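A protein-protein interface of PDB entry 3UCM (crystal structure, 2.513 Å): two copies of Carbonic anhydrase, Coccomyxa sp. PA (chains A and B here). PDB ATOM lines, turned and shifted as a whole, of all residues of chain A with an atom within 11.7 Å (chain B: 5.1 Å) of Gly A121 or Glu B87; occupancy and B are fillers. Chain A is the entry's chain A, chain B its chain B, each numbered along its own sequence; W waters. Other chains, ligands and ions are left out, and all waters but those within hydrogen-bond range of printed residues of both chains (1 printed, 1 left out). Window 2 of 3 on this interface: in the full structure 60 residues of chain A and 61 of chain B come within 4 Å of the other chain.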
ATOM      1  N   ALA A  48     -18.974 -16.317  27.559  1.00  0.00           N
ATOM      2  CA  ALA A  48     -18.690 -16.685  26.147  1.00  0.00           C
ATOM      3  C   ALA A  48     -17.838 -17.980  25.933  1.00  0.00           C
ATOM      4  O   ALA A  48     -17.711 -18.463  24.782  1.00  0.00           O
ATOM      5  CB  ALA A  48     -17.938 -15.579  25.470  1.00  0.00           C
ATOM      6  N   ASN A  70     -20.868 -12.995  27.321  1.00  0.00           N
ATOM      7  CA  ASN A  70     -19.665 -12.153  27.237  1.00  0.00           C
ATOM      8  C   ASN A  70     -18.496 -12.733  28.067  1.00  0.00           C
ATOM      9  O   ASN A  70     -18.720 -13.639  28.908  1.00  0.00           O
ATOM     10  CB  ASN A  70     -20.015 -10.695  27.589  1.00  0.00           C
ATOM     11  CG  ASN A  70     -20.264 -10.499  29.053  1.00  0.00           C
ATOM     12  OD1 ASN A  70     -19.348 -10.655  29.845  1.00  0.00           O
ATOM     13  ND2 ASN A  70     -21.497 -10.121  29.440  1.00  0.00           N
ATOM     14  N   VAL A  71     -17.267 -12.247  27.826  1.00  0.00           N
ATOM     15  CA  VAL A  71     -16.065 -12.781  28.487  1.00  0.00           C
ATOM     16  C   VAL A  71     -16.119 -12.466  29.981  1.00  0.00           C
ATOM     17  O   VAL A  71     -15.910 -11.297  30.371  1.00  0.00           O
ATOM     18  CB  VAL A  71     -14.738 -12.231  27.853  1.00  0.00           C
ATOM     19  CG1 VAL A  71     -13.481 -12.542  28.733  1.00  0.00           C
ATOM     20  CG2 VAL A  71     -14.569 -12.733  26.438  1.00  0.00           C
ATOM     21  N   GLY A 107     -11.244 -18.803  32.379  1.00  0.00           N
ATOM     22  CA  GLY A 107     -10.029 -18.043  32.141  1.00  0.00           C
ATOM     23  C   GLY A 107     -10.138 -16.528  32.101  1.00  0.00           C
ATOM     24  O   GLY A 107      -9.093 -15.864  31.934  1.00  0.00           O
ATOM     25  N   ALA A 108     -11.368 -15.964  32.218  1.00  0.00           N
ATOM     26  CA  ALA A 108     -11.570 -14.489  32.371  1.00  0.00           C
ATOM     27  C   ALA A 108     -11.321 -14.099  33.842  1.00  0.00           C
ATOM     28  O   ALA A 108     -10.811 -13.025  34.152  1.00  0.00           O
ATOM     29  CB  ALA A 108     -13.011 -14.052  31.929  1.00  0.00           C
ATOM     30  N   ALA A 111      -7.259 -14.517  34.283  1.00  0.00           N
ATOM     31  CA  ALA A 111      -6.611 -13.260  33.860  1.00  0.00           C
ATOM     32  C   ALA A 111      -6.828 -12.108  34.890  1.00  0.00           C
ATOM     33  O   ALA A 111      -5.919 -11.294  35.192  1.00  0.00           O
ATOM     34  CB  ALA A 111      -7.126 -12.869  32.502  1.00  0.00           C
ATOM     35  N   TRP A 115      -3.079 -11.095  35.653  1.00  0.00           N
ATOM     36  CA  TRP A 115      -2.512 -10.187  34.678  1.00  0.00           C
ATOM     37  C   TRP A 115      -2.105  -8.871  35.297  1.00  0.00           C
ATOM     38  O   TRP A 115      -2.804  -8.310  36.097  1.00  0.00           O
ATOM     39  CB  TRP A 115      -3.463  -9.916  33.518  1.00  0.00           C
ATOM     40  CG  TRP A 115      -3.635 -11.019  32.549  1.00  0.00           C
ATOM     41  CD1 TRP A 115      -3.113 -12.245  32.628  1.00  0.00           C
ATOM     42  CD2 TRP A 115      -4.420 -10.998  31.359  1.00  0.00           C
ATOM     43  NE1 TRP A 115      -3.505 -12.997  31.566  1.00  0.00           N
ATOM     44  CE2 TRP A 115      -4.312 -12.244  30.772  1.00  0.00           C
ATOM     45  CE3 TRP A 115      -5.198 -10.037  30.736  1.00  0.00           C
ATOM     46  CZ2 TRP A 115      -4.938 -12.557  29.603  1.00  0.00           C
ATOM     47  CZ3 TRP A 115      -5.814 -10.353  29.586  1.00  0.00           C
ATOM     48  CH2 TRP A 115      -5.685 -11.596  29.026  1.00  0.00           C
ATOM     49  N   HIS A 116      -0.950  -8.388  34.896  1.00  0.00           N
ATOM     50  CA  HIS A 116      -0.558  -7.022  35.152  1.00  0.00           C
ATOM     51  C   HIS A 116      -1.399  -6.087  34.277  1.00  0.00           C
ATOM     52  O   HIS A 116      -1.470  -6.240  33.071  1.00  0.00           O
ATOM     53  CB  HIS A 116       0.934  -6.846  34.827  1.00  0.00           C
ATOM     54  CG  HIS A 116       1.570  -5.629  35.456  1.00  0.00           C
ATOM     55  ND1 HIS A 116       1.203  -4.338  35.131  1.00  0.00           N
ATOM     56  CD2 HIS A 116       2.565  -5.513  36.372  1.00  0.00           C
ATOM     57  CE1 HIS A 116       1.937  -3.481  35.820  1.00  0.00           C
ATOM     58  NE2 HIS A 116       2.778  -4.168  36.573  1.00  0.00           N
ATOM     59  N   PRO A 117      -2.018  -5.097  34.865  1.00  0.00           N
ATOM     60  CA  PRO A 117      -2.827  -4.190  34.025  1.00  0.00           C
ATOM     61  C   PRO A 117      -2.106  -3.401  32.883  1.00  0.00           C
ATOM     62  O   PRO A 117      -2.784  -2.695  32.116  1.00  0.00           O
ATOM     63  CB  PRO A 117      -3.492  -3.231  35.036  1.00  0.00           C
ATOM     64  CG  PRO A 117      -2.904  -3.543  36.419  1.00  0.00           C
ATOM     65  CD  PRO A 117      -1.894  -4.678  36.267  1.00  0.00           C
ATOM     66  N   LYS A 118      -0.788  -3.554  32.726  1.00  0.00           N
ATOM     67  CA  LYS A 118      -0.057  -2.944  31.583  1.00  0.00           C
ATOM     68  C   LYS A 118      -0.202  -3.751  30.289  1.00  0.00           C
ATOM     69  O   LYS A 118       0.121  -3.254  29.191  1.00  0.00           O
ATOM     70  CB  LYS A 118       1.431  -2.764  31.893  1.00  0.00           C
ATOM     71  CG  LYS A 118       2.311  -4.055  31.833  1.00  0.00           C
ATOM     72  CD  LYS A 118       3.677  -3.798  32.440  1.00  0.00           C
ATOM     73  CE  LYS A 118       4.690  -4.934  32.207  1.00  0.00           C
ATOM     74  NZ  LYS A 118       5.791  -4.492  31.223  1.00  0.00           N
ATOM     75  N   THR A 119      -0.694  -4.990  30.429  1.00  0.00           N
ATOM     76  CA  THR A 119      -1.025  -5.862  29.299  1.00  0.00           C
ATOM     77  C   THR A 119      -1.766  -5.143  28.147  1.00  0.00           C
ATOM     78  O   THR A 119      -2.832  -4.551  28.344  1.00  0.00           O
ATOM     79  CB  THR A 119      -1.849  -7.071  29.777  1.00  0.00           C
ATOM     80  OG1 THR A 119      -1.173  -7.718  30.877  1.00  0.00           O
ATOM     81  CG2 THR A 119      -2.018  -8.077  28.665  1.00  0.00           C
ATOM     82  N   ALA A 120      -1.179  -5.222  26.955  1.00  0.00           N
ATOM     83  CA  ALA A 120      -1.776  -4.692  25.713  1.00  0.00           C
ATOM     84  C   ALA A 120      -3.169  -5.318  25.377  1.00  0.00           C
ATOM     85  O   ALA A 120      -3.495  -6.404  25.874  1.00  0.00           O
ATOM     86  CB  ALA A 120      -0.784  -4.923  24.540  1.00  0.00           C
ATOM     87  N   GLY A 121      -3.969  -4.635  24.552  1.00  0.00           N
ATOM     88  CA  GLY A 121      -5.241  -5.217  24.044  1.00  0.00           C
ATOM     89  C   GLY A 121      -6.584  -4.904  24.737  1.00  0.00           C
ATOM     90  O   GLY A 121      -6.603  -4.445  25.867  1.00  0.00           O
ATOM     91  N   VAL A 122      -7.701  -5.171  24.048  1.00  0.00           N
ATOM     92  CA  VAL A 122      -9.053  -4.860  24.552  1.00  0.00           C
ATOM     93  C   VAL A 122      -9.545  -5.813  25.620  1.00  0.00           C
ATOM     94  O   VAL A 122     -10.321  -5.380  26.459  1.00  0.00           O
ATOM     95  CB  VAL A 122     -10.156  -4.759  23.431  1.00  0.00           C
ATOM     96  CG1 VAL A 122      -9.995  -3.497  22.645  1.00  0.00           C
ATOM     97  CG2 VAL A 122     -10.080  -5.927  22.487  1.00  0.00           C
ATOM     98  N   THR A 123      -9.131  -7.085  25.604  1.00  0.00           N
ATOM     99  CA  THR A 123      -9.537  -8.012  26.678  1.00  0.00           C
ATOM    100  C   THR A 123      -9.114  -7.525  28.067  1.00  0.00           C
ATOM    101  O   THR A 123      -9.884  -7.635  29.056  1.00  0.00           O
ATOM    102  CB  THR A 123      -9.073  -9.495  26.461  1.00  0.00           C
ATOM    103  OG1 THR A 123      -9.586  -9.959  25.223  1.00  0.00           O
ATOM    104  CG2 THR A 123      -9.683 -10.441  27.534  1.00  0.00           C
ATOM    105  N   ASN A 124      -7.909  -6.968  28.153  1.00  0.00           N
ATOM    106  CA  ASN A 124      -7.418  -6.507  29.456  1.00  0.00           C
ATOM    107  C   ASN A 124      -8.249  -5.299  29.978  1.00  0.00           C
ATOM    108  O   ASN A 124      -8.410  -5.110  31.216  1.00  0.00           O
ATOM    109  CB  ASN A 124      -5.946  -6.176  29.363  1.00  0.00           C
ATOM    110  CG  ASN A 124      -5.380  -5.701  30.675  1.00  0.00           C
ATOM    111  OD1 ASN A 124      -5.397  -6.402  31.721  1.00  0.00           O
ATOM    112  ND2 ASN A 124      -4.875  -4.483  30.651  1.00  0.00           N
ATOM    113  N   LEU A 125      -8.733  -4.467  29.036  1.00  0.00           N
ATOM    114  CA  LEU A 125      -9.622  -3.350  29.361  1.00  0.00           C
ATOM    115  C   LEU A 125     -10.894  -3.986  29.861  1.00  0.00           C
ATOM    116  O   LEU A 125     -11.311  -3.670  30.957  1.00  0.00           O
ATOM    117  CB  LEU A 125      -9.864  -2.428  28.151  1.00  0.00           C
ATOM    118  CG  LEU A 125      -8.610  -1.723  27.513  1.00  0.00           C
ATOM    119  CD1 LEU A 125      -8.997  -0.823  26.351  1.00  0.00           C
ATOM    120  CD2 LEU A 125      -7.862  -0.824  28.498  1.00  0.00           C
ATOM    121  N   TRP A 126     -11.441  -4.950  29.115  1.00  0.00           N
ATOM    122  CA  TRP A 126     -12.741  -5.522  29.425  1.00  0.00           C
ATOM    123  C   TRP A 126     -12.841  -6.183  30.813  1.00  0.00           C
ATOM    124  O   TRP A 126     -13.876  -6.091  31.443  1.00  0.00           O
ATOM    125  CB  TRP A 126     -13.216  -6.473  28.307  1.00  0.00           C
ATOM    126  CG  TRP A 126     -14.501  -7.196  28.635  1.00  0.00           C
ATOM    127  CD1 TRP A 126     -14.628  -8.497  29.114  1.00  0.00           C
ATOM    128  CD2 TRP A 126     -15.850  -6.682  28.545  1.00  0.00           C
ATOM    129  NE1 TRP A 126     -15.972  -8.809  29.321  1.00  0.00           N
ATOM    130  CE2 TRP A 126     -16.736  -7.723  28.979  1.00  0.00           C
ATOM    131  CE3 TRP A 126     -16.399  -5.447  28.153  1.00  0.00           C
ATOM    132  CZ2 TRP A 126     -18.119  -7.560  29.027  1.00  0.00           C
ATOM    133  CZ3 TRP A 126     -17.783  -5.295  28.201  1.00  0.00           C
ATOM    134  CH2 TRP A 126     -18.628  -6.338  28.643  1.00  0.00           C
ATOM    135  N   ILE A 127     -11.785  -6.851  31.279  1.00  0.00           N
ATOM    136  CA  ILE A 127     -11.881  -7.611  32.525  1.00  0.00           C
ATOM    137  C   ILE A 127     -11.499  -6.780  33.739  1.00  0.00           C
ATOM    138  O   ILE A 127     -11.385  -7.345  34.840  1.00  0.00           O
ATOM    139  CB  ILE A 127     -11.004  -8.907  32.589  1.00  0.00           C
ATOM    140  CG1 ILE A 127      -9.497  -8.556  32.577  1.00  0.00           C
ATOM    141  CG2 ILE A 127     -11.372  -9.904  31.508  1.00  0.00           C
ATOM    142  CD1 ILE A 127      -8.648  -9.762  32.617  1.00  0.00           C
ATOM    143  N   SER A 128     -11.343  -5.462  33.565  1.00  0.00           N
ATOM    144  CA  SER A 128     -11.338  -4.515  34.703  1.00  0.00           C
ATOM    145  C   SER A 128     -12.393  -4.799  35.776  1.00  0.00           C
ATOM    146  O   SER A 128     -12.105  -4.613  36.969  1.00  0.00           O
ATOM    147  CB  SER A 128     -11.481  -3.072  34.206  1.00  0.00           C
ATOM    148  OG  SER A 128     -10.471  -2.708  33.252  1.00  0.00           O
ATOM    149  N   ARG A 131     -11.181  -7.344  38.259  1.00  0.00           N
ATOM    150  CA  ARG A 131     -10.211  -6.764  39.196  1.00  0.00           C
ATOM    151  C   ARG A 131     -10.879  -6.043  40.360  1.00  0.00           C
ATOM    152  O   ARG A 131     -10.391  -6.051  41.487  1.00  0.00           O
ATOM    153  CB  ARG A 131      -9.194  -5.838  38.515  1.00  0.00           C
ATOM    154  CG  ARG A 131      -7.913  -6.541  38.160  1.00  0.00           C
ATOM    155  CD  ARG A 131      -7.070  -5.614  37.397  1.00  0.00           C
ATOM    156  NE  ARG A 131      -7.146  -6.033  36.030  1.00  0.00           N
ATOM    157  CZ  ARG A 131      -7.042  -5.249  34.971  1.00  0.00           C
ATOM    158  NH1 ARG A 131      -6.835  -3.955  35.097  1.00  0.00           N
ATOM    159  NH2 ARG A 131      -7.140  -5.787  33.780  1.00  0.00           N
ATOM    160  N   MET B  83     -15.708  -6.755  21.064  1.00  0.00           N
ATOM    161  CA  MET B  83     -14.306  -6.695  20.628  1.00  0.00           C
ATOM    162  C   MET B  83     -13.457  -7.636  21.484  1.00  0.00           C
ATOM    163  O   MET B  83     -12.444  -8.138  21.012  1.00  0.00           O
ATOM    164  CB  MET B  83     -13.728  -5.276  20.696  1.00  0.00           C
ATOM    165  CG  MET B  83     -13.992  -4.436  19.491  1.00  0.00           C
ATOM    166  SD  MET B  83     -13.537  -5.083  17.835  1.00  0.00           S
ATOM    167  CE  MET B  83     -15.130  -5.031  17.040  1.00  0.00           C
ATOM    168  N   SER B  84     -13.832  -7.881  22.736  1.00  0.00           N
ATOM    169  CA  SER B  84     -12.982  -8.823  23.483  1.00  0.00           C
ATOM    170  C   SER B  84     -13.268 -10.243  23.111  1.00  0.00           C
ATOM    171  O   SER B  84     -12.333 -11.058  23.078  1.00  0.00           O
ATOM    172  CB  SER B  84     -12.987  -8.643  24.994  1.00  0.00           C
ATOM    173  OG  SER B  84     -14.324  -8.504  25.424  1.00  0.00           O
ATOM    174  N   CYS B  85     -14.501 -10.553  22.745  1.00  0.00           N
ATOM    175  CA  CYS B  85     -14.759 -11.900  22.257  1.00  0.00           C
ATOM    176  C   CYS B  85     -13.908 -12.162  20.986  1.00  0.00           C
ATOM    177  O   CYS B  85     -13.371 -13.263  20.774  1.00  0.00           O
ATOM    178  CB  CYS B  85     -16.241 -12.127  21.997  1.00  0.00           C
ATOM    179  SG  CYS B  85     -17.198 -12.270  23.475  1.00  0.00           S
ATOM    180  N   LEU B  86     -13.769 -11.129  20.178  1.00  0.00           N
ATOM    181  CA  LEU B  86     -13.054 -11.243  18.948  1.00  0.00           C
ATOM    182  C   LEU B  86     -11.553 -11.293  19.208  1.00  0.00           C
ATOM    183  O   LEU B  86     -10.840 -12.055  18.565  1.00  0.00           O
ATOM    184  CB  LEU B  86     -13.421 -10.075  18.043  1.00  0.00           C
ATOM    185  CG  LEU B  86     -13.150  -9.915  16.550  1.00  0.00           C
ATOM    186  CD1 LEU B  86     -13.317 -11.161  15.636  1.00  0.00           C
ATOM    187  CD2 LEU B  86     -14.012  -8.702  16.029  1.00  0.00           C
ATOM    188  N   GLU B  87     -11.051 -10.500  20.142  1.00  0.00           N
ATOM    189  CA  GLU B  87      -9.608 -10.508  20.342  1.00  0.00           C
ATOM    190  C   GLU B  87      -9.144 -11.851  20.998  1.00  0.00           C
ATOM    191  O   GLU B  87      -8.128 -12.436  20.582  1.00  0.00           O
ATOM    192  CB  GLU B  87      -9.132  -9.242  21.089  1.00  0.00           C
ATOM    193  CG  GLU B  87      -7.698  -9.359  21.685  1.00  0.00           C
ATOM    194  CD  GLU B  87      -7.312  -8.243  22.687  1.00  0.00           C
ATOM    195  OE1 GLU B  87      -6.903  -7.165  22.195  1.00  0.00           O
ATOM    196  OE2 GLU B  87      -7.365  -8.482  23.916  1.00  0.00           O
ATOM    197  N   TYR B  88      -9.914 -12.333  21.989  1.00  0.00           N
ATOM    198  CA  TYR B  88      -9.538 -13.531  22.761  1.00  0.00           C
ATOM    199  C   TYR B  88      -9.496 -14.786  21.935  1.00  0.00           C
ATOM    200  O   TYR B  88      -8.680 -15.679  22.167  1.00  0.00           O
ATOM    201  CB  TYR B  88     -10.489 -13.770  23.946  1.00  0.00           C
ATOM    202  CG  TYR B  88      -9.962 -14.787  24.962  1.00  0.00           C
ATOM    203  CD1 TYR B  88      -9.014 -14.426  25.925  1.00  0.00           C
ATOM    204  CD2 TYR B  88     -10.387 -16.106  24.936  1.00  0.00           C
ATOM    205  CE1 TYR B  88      -8.560 -15.348  26.859  1.00  0.00           C
ATOM    206  CE2 TYR B  88      -9.928 -17.022  25.839  1.00  0.00           C
ATOM    207  CZ  TYR B  88      -9.044 -16.651  26.808  1.00  0.00           C
ATOM    208  OH  TYR B  88      -8.603 -17.623  27.712  1.00  0.00           O
ATOM    209  N   THR B  89     -10.394 -14.876  20.975  1.00  0.00           N
ATOM    210  CA  THR B  89     -10.447 -16.088  20.168  1.00  0.00           C
ATOM    211  C   THR B  89      -9.351 -16.083  19.117  1.00  0.00           C
ATOM    212  O   THR B  89      -8.618 -17.063  18.976  1.00  0.00           O
ATOM    213  CB  THR B  89     -11.787 -16.215  19.502  1.00  0.00           C
ATOM    214  OG1 THR B  89     -12.025 -14.998  18.806  1.00  0.00           O
ATOM    215  CG2 THR B  89     -12.864 -16.464  20.558  1.00  0.00           C
ATOM    216  N   VAL B  90      -9.287 -14.982  18.377  1.00  0.00           N
ATOM    217  CA  VAL B  90      -8.313 -14.778  17.330  1.00  0.00           C
ATOM    218  C   VAL B  90      -6.908 -14.800  17.936  1.00  0.00           C
ATOM    219  O   VAL B  90      -6.118 -15.647  17.569  1.00  0.00           O
ATOM    220  CB  VAL B  90      -8.598 -13.475  16.494  1.00  0.00           C
ATOM    221  CG1 VAL B  90      -7.643 -13.347  15.309  1.00  0.00           C
ATOM    222  CG2 VAL B  90     -10.006 -13.509  15.975  1.00  0.00           C
ATOM    223  N   ASP B  91      -6.600 -13.910  18.884  1.00  0.00           N
ATOM    224  CA  ASP B  91      -5.217 -13.801  19.363  1.00  0.00           C
ATOM    225  C   ASP B  91      -4.757 -14.926  20.317  1.00  0.00           C
ATOM    226  O   ASP B  91      -3.634 -15.427  20.161  1.00  0.00           O
ATOM    227  CB  ASP B  91      -4.900 -12.408  19.900  1.00  0.00           C
ATOM    228  CG  ASP B  91      -4.868 -11.353  18.802  1.00  0.00           C
ATOM    229  OD1 ASP B  91      -4.798 -11.707  17.611  1.00  0.00           O
ATOM    230  OD2 ASP B  91      -4.915 -10.142  19.106  1.00  0.00           O
ATOM    231  N   HIS B  92      -5.589 -15.347  21.272  1.00  0.00           N
ATOM    232  CA  HIS B  92      -5.091 -16.320  22.257  1.00  0.00           C
ATOM    233  C   HIS B  92      -5.537 -17.740  22.019  1.00  0.00           C
ATOM    234  O   HIS B  92      -4.734 -18.662  22.152  1.00  0.00           O
ATOM    235  CB  HIS B  92      -5.376 -15.934  23.730  1.00  0.00           C
ATOM    236  CG  HIS B  92      -5.119 -17.061  24.700  1.00  0.00           C
ATOM    237  ND1 HIS B  92      -3.892 -17.273  25.297  1.00  0.00           N
ATOM    238  CD2 HIS B  92      -5.931 -18.056  25.144  1.00  0.00           C
ATOM    239  CE1 HIS B  92      -3.965 -18.344  26.069  1.00  0.00           C
ATOM    240  NE2 HIS B  92      -5.187 -18.843  25.988  1.00  0.00           N
ATOM    241  N   ILE B 170      -8.307  -6.260  14.912  1.00  0.00           N
ATOM    242  CA  ILE B 170      -7.887  -7.589  15.313  1.00  0.00           C
ATOM    243  C   ILE B 170      -7.660  -8.441  14.038  1.00  0.00           C
ATOM    244  O   ILE B 170      -6.615  -9.089  13.878  1.00  0.00           O
ATOM    245  CB  ILE B 170      -8.982  -8.311  16.131  1.00  0.00           C
ATOM    246  CG1 ILE B 170      -9.488  -7.524  17.364  1.00  0.00           C
ATOM    247  CG2 ILE B 170      -8.523  -9.689  16.502  1.00  0.00           C
ATOM    248  CD1 ILE B 170      -8.431  -7.027  18.325  1.00  0.00           C
HETATM  249  O   HOH W   1     -17.108  -9.614  26.232  1.00  0.00           O
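Ala A48 touches Cys B85 (CB to SG, 3.9 Å).
SG of Cys B85 touches CG2 of Val A71, 3.99 Å away.
Glu B87 touches Gly A121 (OE1 to CA, 3.2 Å).
CG2 of Val A122 touches O of Met B83, at 3.6 Å.
Thr A123 touches Ser B84 (OG1 to CB, 3.7 Å).
OG of Ser B84 touches CG of Trp A126, at 3.5 Å.
No position is printed for both chains.
Trp A115 touches none of the printed residues of chain B.
Pro A117 touches none of the printed residues of chain B.
Gly A121 touches just one residue of chain B: Glu B87 (3.2 Å).
Of the printed residues of chain B, Val A122 touches Met B83 (3.6 Å) and Glu B87 (2.8 Å).
Of the printed residues of chain A, Met B83 touches Val A122.
Of chain A, only Thr A123 and Trp A126 come within 4 Å of Ser B84.
Printed residues of chain A within 4 Å of Cys B85: Ala A48 and Val A71.
No residue of chain A comes within 4 Å of Leu B86.
Glu B87 touches just these residues of chain A: Gly A121, Val A122 and Thr A123.
Thr B89 touches none of the printed residues of chain A.
No residue of chain A comes within 4 Å of Val B90.
No residue of chain A comes within 4 Å of Ile B170.
The nearest printed residue of chain B that does not touch Gly A121 is Ile B170 (6.8 Å).
The nearest residue of chain A that does not touch Glu B87 is Asn A124 (4.5 Å).
The nearest printed residue of chain B that does not touch Trp A126 is Cys B85 (6.7 Å).
The backbone carbonyl oxygen (O) of Val A71 sits at hydrogen-bond distance from the indole nitrogen (NE1) of Trp A126.
O of Asn A70 sits at hydrogen-bond distance from N of Ala A48, 3.0 Å away.
The side-chain hydroxyl (OG1) of Thr B89 lies within hydrogen-bond range of the backbone carbonyl oxygen (O) of Cys B85, at 2.9 Å.
OE2 of Glu B87 lies within hydrogen-bond range of N of Thr A123 (2.8 Å).
The backbone NH (N) of Val A122 is in hydrogen-bond range of the side-chain carboxylate (OE1) of Glu B87 (2.8 Å).
Hydrophobic or aromatic side chains of chain A within 4 Å of the printed part of chain B: Ala A48, Val A71, Val A122 and Trp A126.
Water W1 lies within hydrogen-bond range of the backbone NH (N) of Val A71, the side-chain hydroxyl (OG) of Ser B84 and the indole nitrogen (NE1) of Trp A126.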
